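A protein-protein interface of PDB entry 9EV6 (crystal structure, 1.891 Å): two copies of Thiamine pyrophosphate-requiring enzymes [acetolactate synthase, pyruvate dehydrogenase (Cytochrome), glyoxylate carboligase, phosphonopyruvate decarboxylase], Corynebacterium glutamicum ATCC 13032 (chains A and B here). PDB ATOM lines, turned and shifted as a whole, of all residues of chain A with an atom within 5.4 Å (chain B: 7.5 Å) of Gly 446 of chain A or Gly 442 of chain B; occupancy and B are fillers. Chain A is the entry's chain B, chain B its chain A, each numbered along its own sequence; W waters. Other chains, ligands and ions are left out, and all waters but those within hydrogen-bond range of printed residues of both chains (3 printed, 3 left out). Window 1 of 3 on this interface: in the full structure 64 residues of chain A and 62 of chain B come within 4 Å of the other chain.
OE1 of Glu 447 of chain A sits at hydrogen-bond distance from N of Arg 49 of chain A. N of Arg 49 of chain A is in hydrogen-bond range of OG1 of Thr 450 of chain A (3.4 Å).
Of the 17 printed residues of chain B, 5 touch a printed residue of chain A. Printed residues of chain B that touch a printed residue of chain A: Gly 442, Met 443, Leu 445, Gly 446 and Val 490. Hydrophobic or aromatic side chains of chain B within 4 Å of the printed part of chain A: Met 443, Leu 445 and Val 490. Of the 8 printed residues of chain A, 4 touch a printed residue of chain B. Among the printed residues, 7 pairs touch across the chains.
Leu 445 of chain A touches Gly 446 of chain B, and with the chains exchanged Gly 446 of chain A touches Leu 445 of chain B. Of the 7 pairs that touch across the chains among the printed residues, 2 have their exchanged pair printed and touching as well.
Gly 446 of chain A touches two residues of chain B. Of chain A, only Arg 49 and Gly 446 come within 4 Å of Gly 442 of chain B. Of the printed residues of chain B, Leu 449 of chain A touches Val 490 (3.9 Å). Of the printed residues of chain A, Leu 445 of chain B touches Gly 446. Of the printed residues of chain A, Met 443 of chain B touches Arg 49 (3.4 Å). Of the printed residues of chain A, Gly 446 of chain B touches Leu 445 (3.6 Å). Of the printed residues of chain A, Val 490 of chain B touches Arg 49 and Leu 449. Gly 440 of chain B touches none of the printed residues of chain A. Glu 447 of chain A touches none of the printed residues of chain B.
Water W1 bridges O of Gly 439 of chain B (2.7 Å) and O of Arg 49 of chain A (2.7 Å). Water W3 bridges O of Asp 438 of chain B (2.8 Å) and NE of Arg 49 of chain A (2.8 Å). Water W2 bridges OD2 of Asp 438 of chain B (2.8 Å) and NH2 of Arg 49 of chain A (3.1 Å).
Among the printed residues, merely in contact across the chains: Arg 49 of chain A with Gly 442 of chain B (3.7 Å), Arg 49 of chain A with Met 443 of chain B (3.4 Å), Arg 49 of chain A with Val 490 of chain B (3.6 Å), Leu 445 of chain A with Gly 446 of chain B (3.6 Å), Gly 446 of chain A with Gly 442 of chain B (3.2 Å), Gly 446 of chain A with Leu 445 of chain B (3.7 Å) and Leu 449 of chain A with Val 490 of chain B (3.9 Å).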
ATOM      1  N   ARG A  49      30.402  -3.703  -0.848  1.00  0.00           N
ATOM      2  CA  ARG A  49      29.435  -4.068   0.190  1.00  0.00           C
ATOM      3  C   ARG A  49      28.675  -5.353  -0.155  1.00  0.00           C
ATOM      4  O   ARG A  49      28.286  -6.099   0.737  1.00  0.00           O
ATOM      5  CB  ARG A  49      28.452  -2.909   0.447  1.00  0.00           C
ATOM      6  CG  ARG A  49      28.653  -2.234   1.809  1.00  0.00           C
ATOM      7  CD  ARG A  49      30.045  -1.682   2.027  1.00  0.00           C
ATOM      8  NE  ARG A  49      30.205  -1.207   3.408  1.00  0.00           N
ATOM      9  CZ  ARG A  49      31.219  -0.466   3.839  1.00  0.00           C
ATOM     10  NH1 ARG A  49      32.171  -0.077   2.997  1.00  0.00           N
ATOM     11  NH2 ARG A  49      31.274  -0.077   5.105  1.00  0.00           N
ATOM     12  N   LEU A 444      20.763  -1.725  -4.894  1.00  0.00           N
ATOM     13  CA  LEU A 444      22.116  -1.968  -4.384  1.00  0.00           C
ATOM     14  C   LEU A 444      22.629  -0.687  -3.653  1.00  0.00           C
ATOM     15  O   LEU A 444      23.763  -0.248  -3.858  1.00  0.00           O
ATOM     16  CB  LEU A 444      23.088  -2.386  -5.523  1.00  0.00           C
ATOM     17  CG  LEU A 444      22.915  -3.811  -6.082  1.00  0.00           C
ATOM     18  CD1 LEU A 444      23.842  -4.046  -7.262  1.00  0.00           C
ATOM     19  CD2 LEU A 444      23.136  -4.881  -4.993  1.00  0.00           C
ATOM     20  N   LEU A 445      21.782  -0.122  -2.792  1.00  0.00           N
ATOM     21  CA  LEU A 445      22.028   1.136  -2.083  1.00  0.00           C
ATOM     22  C   LEU A 445      23.325   1.165  -1.281  1.00  0.00           C
ATOM     23  O   LEU A 445      23.975   2.208  -1.208  1.00  0.00           O
ATOM     24  CB  LEU A 445      20.855   1.437  -1.151  1.00  0.00           C
ATOM     25  CG  LEU A 445      20.789   2.850  -0.584  1.00  0.00           C
ATOM     26  CD1 LEU A 445      20.727   3.908  -1.702  1.00  0.00           C
ATOM     27  CD2 LEU A 445      19.608   2.994   0.402  1.00  0.00           C
ATOM     28  N   GLY A 446      23.725   0.020  -0.741  1.00  0.00           N
ATOM     29  CA  GLY A 446      24.941  -0.060   0.044  1.00  0.00           C
ATOM     30  C   GLY A 446      26.205   0.267  -0.718  1.00  0.00           C
ATOM     31  O   GLY A 446      27.236   0.524  -0.093  1.00  0.00           O
ATOM     32  N   GLU A 447      26.161   0.251  -2.068  1.00  0.00           N
ATOM     33  CA  GLU A 447      27.358   0.600  -2.846  1.00  0.00           C
ATOM     34  C   GLU A 447      27.679   2.090  -2.778  1.00  0.00           C
ATOM     35  O   GLU A 447      28.788   2.459  -3.155  1.00  0.00           O
ATOM     36  CB  GLU A 447      27.295   0.095  -4.294  1.00  0.00           C
ATOM     37  CG  GLU A 447      27.233  -1.428  -4.382  1.00  0.00           C
ATOM     38  CD  GLU A 447      28.192  -2.192  -3.472  1.00  0.00           C
ATOM     39  OE1 GLU A 447      29.400  -1.856  -3.438  1.00  0.00           O
ATOM     40  OE2 GLU A 447      27.724  -3.119  -2.778  1.00  0.00           O
ATOM     41  N   LEU A 448      26.789   2.935  -2.185  1.00  0.00           N
ATOM     42  CA  LEU A 448      27.132   4.316  -1.881  1.00  0.00           C
ATOM     43  C   LEU A 448      28.281   4.325  -0.836  1.00  0.00           C
ATOM     44  O   LEU A 448      29.144   5.186  -0.883  1.00  0.00           O
ATOM     45  CB  LEU A 448      25.907   5.072  -1.334  1.00  0.00           C
ATOM     46  CG  LEU A 448      24.847   5.481  -2.359  1.00  0.00           C
ATOM     47  CD1 LEU A 448      23.685   6.186  -1.672  1.00  0.00           C
ATOM     48  CD2 LEU A 448      25.430   6.376  -3.406  1.00  0.00           C
ATOM     49  N   LEU A 449      28.317   3.331   0.070  1.00  0.00           N
ATOM     50  CA  LEU A 449      29.388   3.213   1.070  1.00  0.00           C
ATOM     51  C   LEU A 449      30.715   2.826   0.399  1.00  0.00           C
ATOM     52  O   LEU A 449      31.766   3.201   0.891  1.00  0.00           O
ATOM     53  CB  LEU A 449      29.002   2.167   2.145  1.00  0.00           C
ATOM     54  CG  LEU A 449      27.611   2.397   2.787  1.00  0.00           C
ATOM     55  CD1 LEU A 449      27.231   1.228   3.745  1.00  0.00           C
ATOM     56  CD2 LEU A 449      27.550   3.746   3.490  1.00  0.00           C
ATOM     57  N   THR A 450      30.665   2.105  -0.735  1.00  0.00           N
ATOM     58  CA  THR A 450      31.853   1.721  -1.510  1.00  0.00           C
ATOM     59  C   THR A 450      32.418   2.952  -2.216  1.00  0.00           C
ATOM     60  O   THR A 450      33.640   3.156  -2.233  1.00  0.00           O
ATOM     61  CB  THR A 450      31.493   0.614  -2.516  1.00  0.00           C
ATOM     62  OG1 THR A 450      30.949  -0.508  -1.806  1.00  0.00           O
ATOM     63  CG2 THR A 450      32.704   0.161  -3.344  1.00  0.00           C
ATOM     64  N   ASP B 383      21.899 -11.872  11.931  1.00  0.00           N
ATOM     65  CA  ASP B 383      22.792 -11.707  10.771  1.00  0.00           C
ATOM     66  C   ASP B 383      23.983 -12.637  10.905  1.00  0.00           C
ATOM     67  O   ASP B 383      24.512 -12.780  12.007  1.00  0.00           O
ATOM     68  CB  ASP B 383      23.288 -10.257  10.665  1.00  0.00           C
ATOM     69  CG  ASP B 383      22.870  -9.518   9.393  1.00  0.00           C
ATOM     70  OD1 ASP B 383      22.338 -10.182   8.461  1.00  0.00           O
ATOM     71  OD2 ASP B 383      23.074  -8.262   9.329  1.00  0.00           O
ATOM     72  N   MET B 413      25.537 -13.788   4.780  1.00  0.00           N
ATOM     73  CA  MET B 413      25.405 -12.470   5.398  1.00  0.00           C
ATOM     74  C   MET B 413      24.101 -11.838   4.909  1.00  0.00           C
ATOM     75  O   MET B 413      23.512 -12.307   3.926  1.00  0.00           O
ATOM     76  CB  MET B 413      26.574 -11.557   4.936  1.00  0.00           C
ATOM     77  CG  MET B 413      27.899 -11.771   5.634  1.00  0.00           C
ATOM     78  SD  MET B 413      29.193 -10.841   4.742  1.00  0.00           S
ATOM     79  CE  MET B 413      28.663  -9.143   5.059  1.00  0.00           C
ATOM     80  N   ALA B 414      23.692 -10.731   5.530  1.00  0.00           N
ATOM     81  CA  ALA B 414      22.594  -9.855   5.123  1.00  0.00           C
ATOM     82  C   ALA B 414      21.193 -10.425   5.285  1.00  0.00           C
ATOM     83  O   ALA B 414      20.262  -9.746   4.874  1.00  0.00           O
ATOM     84  CB  ALA B 414      22.772  -9.379   3.676  1.00  0.00           C
ATOM     85  N   CYS B 436      21.549  -7.118  13.508  1.00  0.00           N
ATOM     86  CA  CYS B 436      22.280  -6.863  12.262  1.00  0.00           C
ATOM     87  C   CYS B 436      23.753  -6.659  12.496  1.00  0.00           C
ATOM     88  O   CYS B 436      24.160  -6.054  13.493  1.00  0.00           O
ATOM     89  CB  CYS B 436      21.710  -5.639  11.543  1.00  0.00           C
ATOM     90  SG  CYS B 436      19.928  -5.698  11.227  1.00  0.00           S
ATOM     91  N   GLY B 437      24.537  -7.053  11.519  1.00  0.00           N
ATOM     92  CA  GLY B 437      25.942  -6.697  11.447  1.00  0.00           C
ATOM     93  C   GLY B 437      26.054  -5.486  10.529  1.00  0.00           C
ATOM     94  O   GLY B 437      25.169  -5.261   9.677  1.00  0.00           O
ATOM     95  N   ASP B 438      27.126  -4.681  10.675  1.00  0.00           N
ATOM     96  CA  ASP B 438      27.313  -3.540   9.771  1.00  0.00           C
ATOM     97  C   ASP B 438      27.574  -4.043   8.320  1.00  0.00           C
ATOM     98  O   ASP B 438      27.127  -3.421   7.336  1.00  0.00           O
ATOM     99  CB  ASP B 438      28.452  -2.615  10.259  1.00  0.00           C
ATOM    100  CG  ASP B 438      29.787  -3.321  10.314  1.00  0.00           C
ATOM    101  OD1 ASP B 438      29.895  -4.327  11.059  1.00  0.00           O
ATOM    102  OD2 ASP B 438      30.722  -2.884   9.588  1.00  0.00           O
ATOM    103  N   GLY B 439      28.269  -5.173   8.197  1.00  0.00           N
ATOM    104  CA  GLY B 439      28.534  -5.761   6.896  1.00  0.00           C
ATOM    105  C   GLY B 439      27.250  -6.277   6.275  1.00  0.00           C
ATOM    106  O   GLY B 439      26.953  -5.971   5.117  1.00  0.00           O
ATOM    107  N   GLY B 440      26.475  -7.035   7.059  1.00  0.00           N
ATOM    108  CA  GLY B 440      25.215  -7.562   6.560  1.00  0.00           C
ATOM    109  C   GLY B 440      24.218  -6.485   6.154  1.00  0.00           C
ATOM    110  O   GLY B 440      23.582  -6.588   5.102  1.00  0.00           O
ATOM    111  N   LEU B 441      24.064  -5.434   6.988  1.00  0.00           N
ATOM    112  CA  LEU B 441      23.118  -4.362   6.679  1.00  0.00           C
ATOM    113  C   LEU B 441      23.558  -3.586   5.436  1.00  0.00           C
ATOM    114  O   LEU B 441      22.736  -3.330   4.558  1.00  0.00           O
ATOM    115  CB  LEU B 441      22.924  -3.411   7.866  1.00  0.00           C
ATOM    116  CG  LEU B 441      21.933  -2.259   7.649  1.00  0.00           C
ATOM    117  CD1 LEU B 441      20.538  -2.761   7.256  1.00  0.00           C
ATOM    118  CD2 LEU B 441      21.851  -1.399   8.883  1.00  0.00           C
ATOM    119  N   GLY B 442      24.841  -3.261   5.342  1.00  0.00           N
ATOM    120  CA  GLY B 442      25.367  -2.560   4.173  1.00  0.00           C
ATOM    121  C   GLY B 442      25.172  -3.324   2.875  1.00  0.00           C
ATOM    122  O   GLY B 442      25.007  -2.721   1.805  1.00  0.00           O
ATOM    123  N   MET B 443      25.183  -4.655   2.954  1.00  0.00           N
ATOM    124  CA  MET B 443      25.038  -5.551   1.811  1.00  0.00           C
ATOM    125  C   MET B 443      23.635  -5.448   1.170  1.00  0.00           C
ATOM    126  O   MET B 443      23.517  -5.598  -0.040  1.00  0.00           O
ATOM    127  CB  MET B 443      25.319  -6.998   2.274  1.00  0.00           C
ATOM    128  CG  MET B 443      25.379  -8.006   1.163  1.00  0.00           C
ATOM    129  SD  MET B 443      26.017  -9.585   1.777  1.00  0.00           S
ATOM    130  CE  MET B 443      27.761  -9.341   1.607  1.00  0.00           C
ATOM    131  N   LEU B 444      22.576  -5.197   1.976  1.00  0.00           N
ATOM    132  CA  LEU B 444      21.216  -5.037   1.438  1.00  0.00           C
ATOM    133  C   LEU B 444      20.590  -3.771   2.057  1.00  0.00           C
ATOM    134  O   LEU B 444      19.433  -3.769   2.487  1.00  0.00           O
ATOM    135  CB  LEU B 444      20.335  -6.280   1.695  1.00  0.00           C
ATOM    136  CG  LEU B 444      20.625  -7.534   0.833  1.00  0.00           C
ATOM    137  CD1 LEU B 444      19.756  -8.699   1.272  1.00  0.00           C
ATOM    138  CD2 LEU B 444      20.434  -7.262  -0.656  1.00  0.00           C
ATOM    139  N   LEU B 445      21.358  -2.683   2.057  1.00  0.00           N
ATOM    140  CA  LEU B 445      20.959  -1.427   2.715  1.00  0.00           C
ATOM    141  C   LEU B 445      19.623  -0.857   2.216  1.00  0.00           C
ATOM    142  O   LEU B 445      18.891  -0.243   2.994  1.00  0.00           O
ATOM    143  CB  LEU B 445      22.060  -0.396   2.485  1.00  0.00           C
ATOM    144  CG  LEU B 445      21.965   0.893   3.292  1.00  0.00           C
ATOM    145  CD1 LEU B 445      22.077   0.610   4.762  1.00  0.00           C
ATOM    146  CD2 LEU B 445      23.086   1.875   2.854  1.00  0.00           C
ATOM    147  N   GLY B 446      19.307  -1.082   0.939  1.00  0.00           N
ATOM    148  CA  GLY B 446      18.070  -0.573   0.366  1.00  0.00           C
ATOM    149  C   GLY B 446      16.807  -1.122   0.999  1.00  0.00           C
ATOM    150  O   GLY B 446      15.738  -0.544   0.812  1.00  0.00           O
ATOM    151  N   VAL B 462      21.883  -2.667  15.113  1.00  0.00           N
ATOM    152  CA  VAL B 462      23.132  -2.824  14.376  1.00  0.00           C
ATOM    153  C   VAL B 462      24.326  -2.924  15.330  1.00  0.00           C
ATOM    154  O   VAL B 462      24.609  -1.981  16.061  1.00  0.00           O
ATOM    155  CB  VAL B 462      23.374  -1.673  13.369  1.00  0.00           C
ATOM    156  CG1 VAL B 462      24.540  -2.007  12.442  1.00  0.00           C
ATOM    157  CG2 VAL B 462      22.108  -1.354  12.570  1.00  0.00           C
ATOM    158  N   VAL B 490      30.771   3.901   9.534  1.00  0.00           N
ATOM    159  CA  VAL B 490      29.547   4.280   8.838  1.00  0.00           C
ATOM    160  C   VAL B 490      28.494   4.661   9.882  1.00  0.00           C
ATOM    161  O   VAL B 490      28.344   3.959  10.896  1.00  0.00           O
ATOM    162  CB  VAL B 490      29.048   3.126   7.905  1.00  0.00           C
ATOM    163  CG1 VAL B 490      27.666   3.423   7.343  1.00  0.00           C
ATOM    164  CG2 VAL B 490      30.036   2.881   6.766  1.00  0.00           C
ATOM    165  N   PHE B 492      24.967   4.458  10.555  1.00  0.00           N
ATOM    166  CA  PHE B 492      23.706   3.874  10.132  1.00  0.00           C
ATOM    167  C   PHE B 492      22.506   4.624  10.724  1.00  0.00           C
ATOM    168  O   PHE B 492      21.453   4.637  10.096  1.00  0.00           O
ATOM    169  CB  PHE B 492      23.643   2.377  10.461  1.00  0.00           C
ATOM    170  CG  PHE B 492      24.586   1.572   9.611  1.00  0.00           C
ATOM    171  CD1 PHE B 492      24.267   1.262   8.293  1.00  0.00           C
ATOM    172  CD2 PHE B 492      25.794   1.118  10.123  1.00  0.00           C
ATOM    173  CE1 PHE B 492      25.145   0.536   7.502  1.00  0.00           C
ATOM    174  CE2 PHE B 492      26.671   0.385   9.327  1.00  0.00           C
ATOM    175  CZ  PHE B 492      26.331   0.088   8.029  1.00  0.00           C
HETATM  176  O   HOH W   1      28.991  -5.812   3.359  1.00  0.00           O
HETATM  177  O   HOH W   2      30.540  -0.492   8.131  1.00  0.00           O
HETATM  178  O   HOH W   3      28.985  -1.990   5.846  1.00  0.00           O
